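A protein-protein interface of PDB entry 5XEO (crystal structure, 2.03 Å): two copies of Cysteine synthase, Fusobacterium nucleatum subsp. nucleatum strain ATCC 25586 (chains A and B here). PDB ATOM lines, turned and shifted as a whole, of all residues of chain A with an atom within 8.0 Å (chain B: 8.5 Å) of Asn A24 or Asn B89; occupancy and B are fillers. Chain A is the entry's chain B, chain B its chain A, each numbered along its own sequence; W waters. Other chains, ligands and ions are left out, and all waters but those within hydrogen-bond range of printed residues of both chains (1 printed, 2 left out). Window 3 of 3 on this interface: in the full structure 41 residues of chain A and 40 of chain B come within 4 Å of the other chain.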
ATOM      1  N   LYS A  21       0.929  28.085 -36.223  1.00  0.00           N
ATOM      2  CA  LYS A  21       1.774  26.910 -36.347  1.00  0.00           C
ATOM      3  C   LYS A  21       0.946  25.648 -36.233  1.00  0.00           C
ATOM      4  O   LYS A  21       0.051  25.580 -35.402  1.00  0.00           O
ATOM      5  CB  LYS A  21       2.890  26.900 -35.286  1.00  0.00           C
ATOM      6  CG  LYS A  21       3.759  25.662 -35.446  1.00  0.00           C
ATOM      7  CD  LYS A  21       5.062  25.762 -34.716  1.00  0.00           C
ATOM      8  CE  LYS A  21       5.882  24.513 -35.005  1.00  0.00           C
ATOM      9  NZ  LYS A  21       7.215  24.602 -34.344  1.00  0.00           N
ATOM     10  N   ILE A  22       1.275  24.650 -37.032  1.00  0.00           N
ATOM     11  CA  ILE A  22       0.637  23.334 -36.967  1.00  0.00           C
ATOM     12  C   ILE A  22       1.370  22.479 -35.916  1.00  0.00           C
ATOM     13  O   ILE A  22       2.578  22.313 -35.990  1.00  0.00           O
ATOM     14  CB  ILE A  22       0.651  22.655 -38.365  1.00  0.00           C
ATOM     15  CG1 ILE A  22      -0.179  23.472 -39.355  1.00  0.00           C
ATOM     16  CG2 ILE A  22       0.196  21.217 -38.308  1.00  0.00           C
ATOM     17  CD1 ILE A  22      -1.655  23.550 -39.052  1.00  0.00           C
ATOM     18  N   ASN A  23       0.634  21.985 -34.921  1.00  0.00           N
ATOM     19  CA  ASN A  23       1.212  21.302 -33.738  1.00  0.00           C
ATOM     20  C   ASN A  23       0.911  19.827 -33.546  1.00  0.00           C
ATOM     21  O   ASN A  23       1.714  19.133 -32.952  1.00  0.00           O
ATOM     22  CB  ASN A  23       0.722  21.975 -32.456  1.00  0.00           C
ATOM     23  CG  ASN A  23       1.086  23.420 -32.411  1.00  0.00           C
ATOM     24  OD1 ASN A  23       2.258  23.758 -32.407  1.00  0.00           O
ATOM     25  ND2 ASN A  23       0.075  24.289 -32.437  1.00  0.00           N
ATOM     26  N   ASN A  24      -0.263  19.373 -33.962  1.00  0.00           N
ATOM     27  CA  ASN A  24      -0.670  17.992 -33.760  1.00  0.00           C
ATOM     28  C   ASN A  24      -0.514  17.128 -35.011  1.00  0.00           C
ATOM     29  O   ASN A  24      -0.220  15.929 -34.891  1.00  0.00           O
ATOM     30  CB  ASN A  24      -2.116  17.935 -33.264  1.00  0.00           C
ATOM     31  CG  ASN A  24      -2.265  18.433 -31.830  1.00  0.00           C
ATOM     32  OD1 ASN A  24      -1.501  18.042 -30.962  1.00  0.00           O
ATOM     33  ND2 ASN A  24      -3.281  19.279 -31.566  1.00  0.00           N
ATOM     34  N   ILE A  25      -0.691  17.706 -36.200  1.00  0.00           N
ATOM     35  CA  ILE A  25      -0.457  16.957 -37.440  1.00  0.00           C
ATOM     36  C   ILE A  25       1.040  16.797 -37.599  1.00  0.00           C
ATOM     37  O   ILE A  25       1.808  17.739 -37.341  1.00  0.00           O
ATOM     38  CB  ILE A  25      -1.115  17.657 -38.663  1.00  0.00           C
ATOM     39  CG1 ILE A  25      -2.625  17.538 -38.549  1.00  0.00           C
ATOM     40  CG2 ILE A  25      -0.650  17.050 -39.988  1.00  0.00           C
ATOM     41  CD1 ILE A  25      -3.397  18.464 -39.475  1.00  0.00           C
ATOM     42  N   ASP A  26       1.476  15.587 -37.965  1.00  0.00           N
ATOM     43  CA  ASP A  26       2.894  15.340 -38.211  1.00  0.00           C
ATOM     44  C   ASP A  26       3.268  16.065 -39.493  1.00  0.00           C
ATOM     45  O   ASP A  26       2.742  15.745 -40.537  1.00  0.00           O
ATOM     46  CB  ASP A  26       3.188  13.836 -38.351  1.00  0.00           C
ATOM     47  CG  ASP A  26       4.702  13.500 -38.393  1.00  0.00           C
ATOM     48  OD1 ASP A  26       5.541  14.404 -38.667  1.00  0.00           O
ATOM     49  OD2 ASP A  26       5.048  12.336 -38.131  1.00  0.00           O
ATOM     50  N   THR A  27       4.179  17.018 -39.407  1.00  0.00           N
ATOM     51  CA  THR A  27       4.610  17.777 -40.589  1.00  0.00           C
ATOM     52  C   THR A  27       6.011  17.399 -41.074  1.00  0.00           C
ATOM     53  O   THR A  27       6.638  18.162 -41.832  1.00  0.00           O
ATOM     54  CB  THR A  27       4.489  19.292 -40.359  1.00  0.00           C
ATOM     55  OG1 THR A  27       5.310  19.678 -39.260  1.00  0.00           O
ATOM     56  CG2 THR A  27       3.063  19.657 -40.032  1.00  0.00           C
ATOM     57  N   GLU A 258      -9.363  16.961 -41.066  1.00  0.00           N
ATOM     58  CA  GLU A 258      -8.162  16.760 -40.254  1.00  0.00           C
ATOM     59  C   GLU A 258      -7.727  18.045 -39.555  1.00  0.00           C
ATOM     60  O   GLU A 258      -7.305  18.022 -38.400  1.00  0.00           O
ATOM     61  CB  GLU A 258      -6.947  16.291 -41.077  1.00  0.00           C
ATOM     62  CG  GLU A 258      -7.033  14.932 -41.753  1.00  0.00           C
ATOM     63  CD  GLU A 258      -6.361  13.828 -40.956  1.00  0.00           C
ATOM     64  OE1 GLU A 258      -5.156  13.968 -40.654  1.00  0.00           O
ATOM     65  OE2 GLU A 258      -7.038  12.836 -40.628  1.00  0.00           O
ATOM     66  N   LEU A 259      -7.746  19.158 -40.282  1.00  0.00           N
ATOM     67  CA  LEU A 259      -7.383  20.440 -39.699  1.00  0.00           C
ATOM     68  C   LEU A 259      -8.304  20.834 -38.561  1.00  0.00           C
ATOM     69  O   LEU A 259      -7.834  21.304 -37.533  1.00  0.00           O
ATOM     70  CB  LEU A 259      -7.318  21.551 -40.758  1.00  0.00           C
ATOM     71  CG  LEU A 259      -6.111  21.511 -41.691  1.00  0.00           C
ATOM     72  CD1 LEU A 259      -6.341  22.418 -42.911  1.00  0.00           C
ATOM     73  CD2 LEU A 259      -4.851  21.919 -40.941  1.00  0.00           C
ATOM     74  N   PHE A 261     -10.322  18.771 -36.656  1.00  0.00           N
ATOM     75  CA  PHE A 261     -10.191  17.747 -35.596  1.00  0.00           C
ATOM     76  C   PHE A 261      -8.883  17.885 -34.811  1.00  0.00           C
ATOM     77  O   PHE A 261      -8.835  17.675 -33.616  1.00  0.00           O
ATOM     78  CB  PHE A 261     -10.093  16.315 -36.208  1.00  0.00           C
ATOM     79  CG  PHE A 261     -11.364  15.730 -36.757  1.00  0.00           C
ATOM     80  CD1 PHE A 261     -12.618  16.228 -36.466  1.00  0.00           C
ATOM     81  CD2 PHE A 261     -11.274  14.567 -37.540  1.00  0.00           C
ATOM     82  CE1 PHE A 261     -13.757  15.611 -36.960  1.00  0.00           C
ATOM     83  CE2 PHE A 261     -12.408  13.944 -38.036  1.00  0.00           C
ATOM     84  CZ  PHE A 261     -13.659  14.470 -37.732  1.00  0.00           C
ATOM     85  N   LYS A 262      -7.791  18.105 -35.528  1.00  0.00           N
ATOM     86  CA  LYS A 262      -6.460  18.054 -34.922  1.00  0.00           C
ATOM     87  C   LYS A 262      -5.904  19.409 -34.544  1.00  0.00           C
ATOM     88  O   LYS A 262      -5.045  19.501 -33.664  1.00  0.00           O
ATOM     89  CB  LYS A 262      -5.522  17.304 -35.865  1.00  0.00           C
ATOM     90  CG  LYS A 262      -5.867  15.824 -35.961  1.00  0.00           C
ATOM     91  CD  LYS A 262      -4.917  15.104 -36.912  1.00  0.00           C
ATOM     92  CE  LYS A 262      -5.336  13.644 -37.114  1.00  0.00           C
ATOM     93  NZ  LYS A 262      -4.423  12.908 -38.025  1.00  0.00           N
ATOM     94  N   GLU A 263      -6.341  20.480 -35.212  1.00  0.00           N
ATOM     95  CA  GLU A 263      -5.759  21.810 -34.933  1.00  0.00           C
ATOM     96  C   GLU A 263      -6.757  22.855 -34.464  1.00  0.00           C
ATOM     97  O   GLU A 263      -6.360  23.972 -34.085  1.00  0.00           O
ATOM     98  CB  GLU A 263      -5.033  22.337 -36.164  1.00  0.00           C
ATOM     99  CG  GLU A 263      -3.962  21.400 -36.707  1.00  0.00           C
ATOM    100  CD  GLU A 263      -2.749  21.229 -35.805  1.00  0.00           C
ATOM    101  OE1 GLU A 263      -2.290  22.201 -35.142  1.00  0.00           O
ATOM    102  OE2 GLU A 263      -2.213  20.100 -35.776  1.00  0.00           O
ATOM    103  N   GLY A 264      -8.037  22.517 -34.489  1.00  0.00           N
ATOM    104  CA  GLY A 264      -9.088  23.492 -34.210  1.00  0.00           C
ATOM    105  C   GLY A 264      -9.169  24.573 -35.281  1.00  0.00           C
ATOM    106  O   GLY A 264      -9.706  25.648 -35.009  1.00  0.00           O
ATOM    107  N   ASN B   8       1.005  30.223 -31.759  1.00  0.00           N
ATOM    108  CA  ASN B   8       1.386  28.803 -31.554  1.00  0.00           C
ATOM    109  C   ASN B   8       0.266  27.856 -31.878  1.00  0.00           C
ATOM    110  O   ASN B   8       0.516  26.730 -32.307  1.00  0.00           O
ATOM    111  CB  ASN B   8       1.797  28.521 -30.128  1.00  0.00           C
ATOM    112  CG  ASN B   8       2.992  29.328 -29.721  1.00  0.00           C
ATOM    113  OD1 ASN B   8       4.054  29.212 -30.331  1.00  0.00           O
ATOM    114  ND2 ASN B   8       2.823  30.169 -28.704  1.00  0.00           N
ATOM    115  N   SER B   9      -0.958  28.283 -31.590  1.00  0.00           N
ATOM    116  CA  SER B   9      -2.148  27.527 -31.900  1.00  0.00           C
ATOM    117  C   SER B   9      -3.307  28.507 -31.969  1.00  0.00           C
ATOM    118  O   SER B   9      -3.165  29.709 -31.665  1.00  0.00           O
ATOM    119  CB  SER B   9      -2.431  26.530 -30.770  1.00  0.00           C
ATOM    120  OG  SER B   9      -2.987  27.215 -29.639  1.00  0.00           O
ATOM    121  N   ILE B  11      -5.577  28.727 -29.922  1.00  0.00           N
ATOM    122  CA  ILE B  11      -5.752  29.257 -28.561  1.00  0.00           C
ATOM    123  C   ILE B  11      -5.196  30.660 -28.398  1.00  0.00           C
ATOM    124  O   ILE B  11      -5.831  31.491 -27.757  1.00  0.00           O
ATOM    125  CB  ILE B  11      -5.193  28.292 -27.475  1.00  0.00           C
ATOM    126  CG1 ILE B  11      -6.090  27.042 -27.432  1.00  0.00           C
ATOM    127  CG2 ILE B  11      -5.165  28.964 -26.108  1.00  0.00           C
ATOM    128  CD1 ILE B  11      -5.633  25.973 -26.455  1.00  0.00           C
ATOM    129  N   GLU B  58      -7.316  21.832 -15.741  1.00  0.00           N
ATOM    130  CA  GLU B  58      -6.004  21.189 -15.961  1.00  0.00           C
ATOM    131  C   GLU B  58      -5.067  21.453 -14.787  1.00  0.00           C
ATOM    132  O   GLU B  58      -4.511  20.537 -14.187  1.00  0.00           O
ATOM    133  CB  GLU B  58      -5.340  21.735 -17.239  1.00  0.00           C
ATOM    134  CG  GLU B  58      -6.008  21.276 -18.509  1.00  0.00           C
ATOM    135  CD  GLU B  58      -5.347  21.871 -19.758  1.00  0.00           C
ATOM    136  OE1 GLU B  58      -5.111  23.077 -19.837  1.00  0.00           O
ATOM    137  OE2 GLU B  58      -5.052  21.109 -20.666  1.00  0.00           O
ATOM    138  N   ILE B  63      -8.432  17.483 -14.960  1.00  0.00           N
ATOM    139  CA  ILE B  63      -8.346  16.955 -16.316  1.00  0.00           C
ATOM    140  C   ILE B  63      -6.997  16.296 -16.549  1.00  0.00           C
ATOM    141  O   ILE B  63      -6.007  16.973 -16.547  1.00  0.00           O
ATOM    142  CB  ILE B  63      -8.585  18.080 -17.349  1.00  0.00           C
ATOM    143  CG1 ILE B  63      -9.997  18.673 -17.160  1.00  0.00           C
ATOM    144  CG2 ILE B  63      -8.394  17.535 -18.760  1.00  0.00           C
ATOM    145  CD1 ILE B  63     -10.221  19.960 -17.931  1.00  0.00           C
ATOM    146  N   ASP B  64      -6.991  14.971 -16.717  1.00  0.00           N
ATOM    147  CA  ASP B  64      -5.845  14.200 -17.170  1.00  0.00           C
ATOM    148  C   ASP B  64      -6.033  13.988 -18.685  1.00  0.00           C
ATOM    149  O   ASP B  64      -7.133  14.189 -19.243  1.00  0.00           O
ATOM    150  CB  ASP B  64      -5.800  12.790 -16.515  1.00  0.00           C
ATOM    151  CG  ASP B  64      -5.897  12.791 -14.956  1.00  0.00           C
ATOM    152  OD1 ASP B  64      -5.469  13.777 -14.313  1.00  0.00           O
ATOM    153  OD2 ASP B  64      -6.375  11.778 -14.387  1.00  0.00           O
ATOM    154  N   LYS B  65      -5.008  13.471 -19.345  1.00  0.00           N
ATOM    155  CA  LYS B  65      -5.105  13.199 -20.795  1.00  0.00           C
ATOM    156  C   LYS B  65      -6.273  12.304 -21.184  1.00  0.00           C
ATOM    157  O   LYS B  65      -6.761  12.395 -22.309  1.00  0.00           O
ATOM    158  CB  LYS B  65      -3.799  12.598 -21.362  1.00  0.00           C
ATOM    159  CG  LYS B  65      -3.433  11.230 -20.784  1.00  0.00           C
ATOM    160  CD  LYS B  65      -2.589  10.391 -21.739  1.00  0.00           C
ATOM    161  CE  LYS B  65      -2.757   8.897 -21.452  1.00  0.00           C
ATOM    162  NZ  LYS B  65      -1.691   8.083 -22.106  1.00  0.00           N
ATOM    163  N   ASP B  66      -6.709  11.418 -20.293  1.00  0.00           N
ATOM    164  CA  ASP B  66      -7.843  10.541 -20.593  1.00  0.00           C
ATOM    165  C   ASP B  66      -9.168  10.959 -19.928  1.00  0.00           C
ATOM    166  O   ASP B  66     -10.113  10.198 -19.923  1.00  0.00           O
ATOM    167  CB  ASP B  66      -7.510   9.053 -20.308  1.00  0.00           C
ATOM    168  CG  ASP B  66      -7.150   8.784 -18.872  1.00  0.00           C
ATOM    169  OD1 ASP B  66      -6.733   9.729 -18.175  1.00  0.00           O
ATOM    170  OD2 ASP B  66      -7.260   7.619 -18.446  1.00  0.00           O
ATOM    171  N   THR B  67      -9.249  12.168 -19.395  1.00  0.00           N
ATOM    172  CA  THR B  67     -10.518  12.670 -18.837  1.00  0.00           C
ATOM    173  C   THR B  67     -11.448  13.062 -19.969  1.00  0.00           C
ATOM    174  O   THR B  67     -11.040  13.788 -20.878  1.00  0.00           O
ATOM    175  CB  THR B  67     -10.280  13.907 -17.969  1.00  0.00           C
ATOM    176  OG1 THR B  67      -9.328  13.574 -16.967  1.00  0.00           O
ATOM    177  CG2 THR B  67     -11.555  14.369 -17.298  1.00  0.00           C
ATOM    178  N   ILE B  69     -14.391  15.322 -21.278  1.00  0.00           N
ATOM    179  CA  ILE B  69     -15.059  16.571 -20.934  1.00  0.00           C
ATOM    180  C   ILE B  69     -16.493  16.372 -21.344  1.00  0.00           C
ATOM    181  O   ILE B  69     -16.748  15.929 -22.463  1.00  0.00           O
ATOM    182  CB  ILE B  69     -14.469  17.791 -21.664  1.00  0.00           C
ATOM    183  CG1 ILE B  69     -12.944  17.810 -21.566  1.00  0.00           C
ATOM    184  CG2 ILE B  69     -15.104  19.075 -21.173  1.00  0.00           C
ATOM    185  CD1 ILE B  69     -12.404  17.784 -20.162  1.00  0.00           C
ATOM    186  N   LEU B  81     -15.727  24.896 -26.435  1.00  0.00           N
ATOM    187  CA  LEU B  81     -15.116  23.695 -25.851  1.00  0.00           C
ATOM    188  C   LEU B  81     -14.536  22.734 -26.900  1.00  0.00           C
ATOM    189  O   LEU B  81     -13.430  22.234 -26.738  1.00  0.00           O
ATOM    190  CB  LEU B  81     -16.124  22.961 -24.981  1.00  0.00           C
ATOM    191  CG  LEU B  81     -16.463  23.666 -23.671  1.00  0.00           C
ATOM    192  CD1 LEU B  81     -17.671  22.969 -23.074  1.00  0.00           C
ATOM    193  CD2 LEU B  81     -15.270  23.649 -22.705  1.00  0.00           C
ATOM    194  N   ALA B  82     -15.292  22.507 -27.969  1.00  0.00           N
ATOM    195  CA  ALA B  82     -14.889  21.640 -29.065  1.00  0.00           C
ATOM    196  C   ALA B  82     -13.566  22.066 -29.683  1.00  0.00           C
ATOM    197  O   ALA B  82     -12.619  21.265 -29.809  1.00  0.00           O
ATOM    198  CB  ALA B  82     -15.999  21.584 -30.108  1.00  0.00           C
ATOM    199  N   MET B  83     -13.454  23.355 -29.984  1.00  0.00           N
ATOM    200  CA  MET B  83     -12.231  23.892 -30.581  1.00  0.00           C
ATOM    201  C   MET B  83     -11.027  23.741 -29.633  1.00  0.00           C
ATOM    202  O   MET B  83      -9.942  23.319 -30.058  1.00  0.00           O
ATOM    203  CB  MET B  83     -12.444  25.365 -30.931  1.00  0.00           C
ATOM    204  CG  MET B  83     -11.248  26.021 -31.577  1.00  0.00           C
ATOM    205  SD  MET B  83     -11.447  27.793 -31.707  1.00  0.00           S
ATOM    206  CE  MET B  83     -11.475  28.207 -29.956  1.00  0.00           C
ATOM    207  N   ILE B  84     -11.228  24.094 -28.368  1.00  0.00           N
ATOM    208  CA  ILE B  84     -10.183  23.998 -27.335  1.00  0.00           C
ATOM    209  C   ILE B  84      -9.764  22.526 -27.176  1.00  0.00           C
ATOM    210  O   ILE B  84      -8.558  22.203 -27.117  1.00  0.00           O
ATOM    211  CB  ILE B  84     -10.666  24.544 -25.953  1.00  0.00           C
ATOM    212  CG1 ILE B  84     -10.950  26.064 -26.011  1.00  0.00           C
ATOM    213  CG2 ILE B  84      -9.646  24.250 -24.867  1.00  0.00           C
ATOM    214  CD1 ILE B  84      -9.753  26.877 -26.394  1.00  0.00           C
ATOM    215  N   CYS B  85     -10.750  21.646 -27.123  1.00  0.00           N
ATOM    216  CA  CYS B  85     -10.466  20.213 -26.933  1.00  0.00           C
ATOM    217  C   CYS B  85      -9.786  19.562 -28.150  1.00  0.00           C
ATOM    218  O   CYS B  85      -8.937  18.658 -27.988  1.00  0.00           O
ATOM    219  CB  CYS B  85     -11.691  19.444 -26.535  1.00  0.00           C
ATOM    220  SG  CYS B  85     -12.278  19.768 -24.855  1.00  0.00           S
ATOM    221  N   ALA B  86     -10.088  20.082 -29.337  1.00  0.00           N
ATOM    222  CA  ALA B  86      -9.375  19.707 -30.550  1.00  0.00           C
ATOM    223  C   ALA B  86      -7.883  20.015 -30.441  1.00  0.00           C
ATOM    224  O   ALA B  86      -7.031  19.148 -30.679  1.00  0.00           O
ATOM    225  CB  ALA B  86      -9.980  20.416 -31.758  1.00  0.00           C
ATOM    226  N   VAL B  87      -7.567  21.227 -30.013  1.00  0.00           N
ATOM    227  CA  VAL B  87      -6.168  21.636 -29.881  1.00  0.00           C
ATOM    228  C   VAL B  87      -5.454  20.809 -28.803  1.00  0.00           C
ATOM    229  O   VAL B  87      -4.324  20.372 -28.986  1.00  0.00           O
ATOM    230  CB  VAL B  87      -6.046  23.139 -29.559  1.00  0.00           C
ATOM    231  CG1 VAL B  87      -4.608  23.522 -29.248  1.00  0.00           C
ATOM    232  CG2 VAL B  87      -6.556  23.952 -30.724  1.00  0.00           C
ATOM    233  N   LYS B  88      -6.121  20.618 -27.679  1.00  0.00           N
ATOM    234  CA  LYS B  88      -5.511  19.975 -26.514  1.00  0.00           C
ATOM    235  C   LYS B  88      -5.598  18.438 -26.513  1.00  0.00           C
ATOM    236  O   LYS B  88      -5.068  17.788 -25.619  1.00  0.00           O
ATOM    237  CB  LYS B  88      -6.124  20.552 -25.254  1.00  0.00           C
ATOM    238  CG  LYS B  88      -5.736  21.999 -24.991  1.00  0.00           C
ATOM    239  CD  LYS B  88      -6.419  22.458 -23.716  1.00  0.00           C
ATOM    240  CE  LYS B  88      -6.041  23.868 -23.320  1.00  0.00           C
ATOM    241  NZ  LYS B  88      -4.696  23.921 -22.731  1.00  0.00           N
ATOM    242  N   ASN B  89      -6.280  17.863 -27.500  1.00  0.00           N
ATOM    243  CA  ASN B  89      -6.458  16.428 -27.617  1.00  0.00           C
ATOM    244  C   ASN B  89      -7.295  15.805 -26.484  1.00  0.00           C
ATOM    245  O   ASN B  89      -7.023  14.677 -26.086  1.00  0.00           O
ATOM    246  CB  ASN B  89      -5.098  15.724 -27.749  1.00  0.00           C
ATOM    247  CG  ASN B  89      -4.368  16.140 -29.011  1.00  0.00           C
ATOM    248  OD1 ASN B  89      -4.861  15.894 -30.100  1.00  0.00           O
ATOM    249  ND2 ASN B  89      -3.234  16.811 -28.870  1.00  0.00           N
ATOM    250  N   TYR B  90      -8.290  16.528 -25.964  1.00  0.00           N
ATOM    251  CA  TYR B  90      -9.215  15.935 -24.995  1.00  0.00           C
ATOM    252  C   TYR B  90     -10.463  15.438 -25.711  1.00  0.00           C
ATOM    253  O   TYR B  90     -10.928  16.054 -26.656  1.00  0.00           O
ATOM    254  CB  TYR B  90      -9.621  16.933 -23.905  1.00  0.00           C
ATOM    255  CG  TYR B  90      -8.475  17.460 -23.068  1.00  0.00           C
ATOM    256  CD1 TYR B  90      -7.518  16.593 -22.543  1.00  0.00           C
ATOM    257  CD2 TYR B  90      -8.377  18.800 -22.745  1.00  0.00           C
ATOM    258  CE1 TYR B  90      -6.465  17.058 -21.792  1.00  0.00           C
ATOM    259  CE2 TYR B  90      -7.322  19.282 -21.972  1.00  0.00           C
ATOM    260  CZ  TYR B  90      -6.375  18.396 -21.493  1.00  0.00           C
ATOM    261  OH  TYR B  90      -5.316  18.795 -20.704  1.00  0.00           O
ATOM    262  N   LYS B  91     -11.014  14.344 -25.218  1.00  0.00           N
ATOM    263  CA  LYS B  91     -12.278  13.821 -25.667  1.00  0.00           C
ATOM    264  C   LYS B  91     -13.435  14.621 -25.065  1.00  0.00           C
ATOM    265  O   LYS B  91     -13.490  14.791 -23.847  1.00  0.00           O
ATOM    266  CB  LYS B  91     -12.360  12.361 -25.229  1.00  0.00           C
ATOM    267  CG  LYS B  91     -13.611  11.622 -25.610  1.00  0.00           C
ATOM    268  CD  LYS B  91     -13.420  10.142 -25.282  1.00  0.00           C
ATOM    269  CE  LYS B  91     -14.743   9.413 -25.271  1.00  0.00           C
ATOM    270  NZ  LYS B  91     -14.547   7.940 -25.248  1.00  0.00           N
ATOM    271  N   LEU B  92     -14.368  15.066 -25.917  1.00  0.00           N
ATOM    272  CA  LEU B  92     -15.456  15.922 -25.525  1.00  0.00           C
ATOM    273  C   LEU B  92     -16.772  15.243 -25.917  1.00  0.00           C
ATOM    274  O   LEU B  92     -16.930  14.783 -27.059  1.00  0.00           O
ATOM    275  CB  LEU B  92     -15.330  17.292 -26.204  1.00  0.00           C
ATOM    276  CG  LEU B  92     -16.483  18.301 -25.951  1.00  0.00           C
ATOM    277  CD1 LEU B  92     -16.593  18.787 -24.517  1.00  0.00           C
ATOM    278  CD2 LEU B  92     -16.345  19.525 -26.846  1.00  0.00           C
ATOM    279  N   TYR B 111     -15.064  19.722 -35.168  1.00  0.00           N
ATOM    280  CA  TYR B 111     -13.946  19.702 -34.209  1.00  0.00           C
ATOM    281  C   TYR B 111     -13.741  18.368 -33.494  1.00  0.00           C
ATOM    282  O   TYR B 111     -12.831  18.258 -32.694  1.00  0.00           O
ATOM    283  CB  TYR B 111     -14.148  20.766 -33.157  1.00  0.00           C
ATOM    284  CG  TYR B 111     -14.111  22.153 -33.687  1.00  0.00           C
ATOM    285  CD1 TYR B 111     -12.933  22.699 -34.169  1.00  0.00           C
ATOM    286  CD2 TYR B 111     -15.259  22.942 -33.689  1.00  0.00           C
ATOM    287  CE1 TYR B 111     -12.891  23.985 -34.647  1.00  0.00           C
ATOM    288  CE2 TYR B 111     -15.224  24.224 -34.160  1.00  0.00           C
ATOM    289  CZ  TYR B 111     -14.051  24.741 -34.626  1.00  0.00           C
ATOM    290  OH  TYR B 111     -14.045  26.003 -35.109  1.00  0.00           O
HETATM  291  O   HOH W   1     -11.091  27.296 -36.127  1.00  0.00           O
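The backbone carbonyl oxygen of Asn B8 is in hydrogen-bond range of the side-chain amide nitrogen of Asn A23 (2.5 Å). ND2 of Asn A24 sits at hydrogen-bond distance from O of Val B87 (3.0 Å). The side-chain amide nitrogen (ND2) of Asn B89 sits at hydrogen-bond distance from the side-chain amide oxygen (OD1) of Asn A24, 3.0 Å away. The backbone carbonyl oxygen (O) of Lys A21 sits close to the backbone carbonyl oxygen (O) of Asn B8 (3.3 Å).
The backbone NH (N) of Ile B11 lies within hydrogen-bond range of the side-chain hydroxyl (OG) of Ser B9 (3.0 Å). O of Lys A21 lies within hydrogen-bond range of ND2 of Asn A23. The side-chain amide nitrogen of Asn A24 is in hydrogen-bond range of the backbone carbonyl oxygen of Lys A262 (2.8 Å). The backbone NH of Ile A25 sits at hydrogen-bond distance from the side-chain carboxylate of Glu A263, at 2.9 Å. NZ of Lys A262 lies within salt-bridge range of OE1 of Glu A258 (2.9 Å). O of Leu A259 sits at hydrogen-bond distance from N of Gly A264 (3.3 Å).
Among the printed residues, pairs that only touch across the chains: Glu A263 with Val B87, Phe A261 with Ala B86, Lys A262 with Ala B86, Gly A264 with Tyr B111, Asn A23 with Ser B9, Gly A264 with Met B83, Phe A261 with Tyr B111, Asn A24 with Ala B86 and Gly A264 with Ala B86.
Asn A24 touches three residues of chain B. Asn B89 touches just one residue of chain A: Asn A24 (3.0 Å). Of the printed residues of chain B, Lys A21 touches Asn B8. Printed residues of chain A within 4 Å of Tyr B111: Phe A261 (3.8 Å) and Gly A264 (3.6 Å). Printed residues of chain B within 4 Å of Phe A261: Ala B86 (3.5 Å) and Tyr B111 (3.8 Å). Printed residues of chain A within 4 Å of Asn B8: Lys A21 (3.3 Å) and Asn A23 (2.5 Å). Ile B69 touches none of the printed residues of chain A. Ile B84 touches none of the printed residues of chain A. The nearest residue of chain A that does not touch Asn B89 is Lys A262 (5.1 Å). The nearest printed residue of chain B that does not touch Lys A21 is Ser B9 (4.6 Å).
Of the 13 printed residues of chain A, 7 touch a printed residue of chain B. Hydrophobic or aromatic side chains of chain A that line the printed part of chain B: Phe A261. Of the 23 printed residues of chain B, 7 touch a printed residue of chain A. Hydrophobic or aromatic side chains of chain B within 4 Å of the printed part of chain A: Met B83, Ala B86, Val B87 and Tyr B111. Among the printed residues, no Asp or Glu carboxylate lies within 4 Å of a Lys or Arg side-chain nitrogen of the other chain.
No position is printed for both chains.
Water W1 lies within hydrogen-bond range of O of Gly A264 and OH of Tyr B111.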
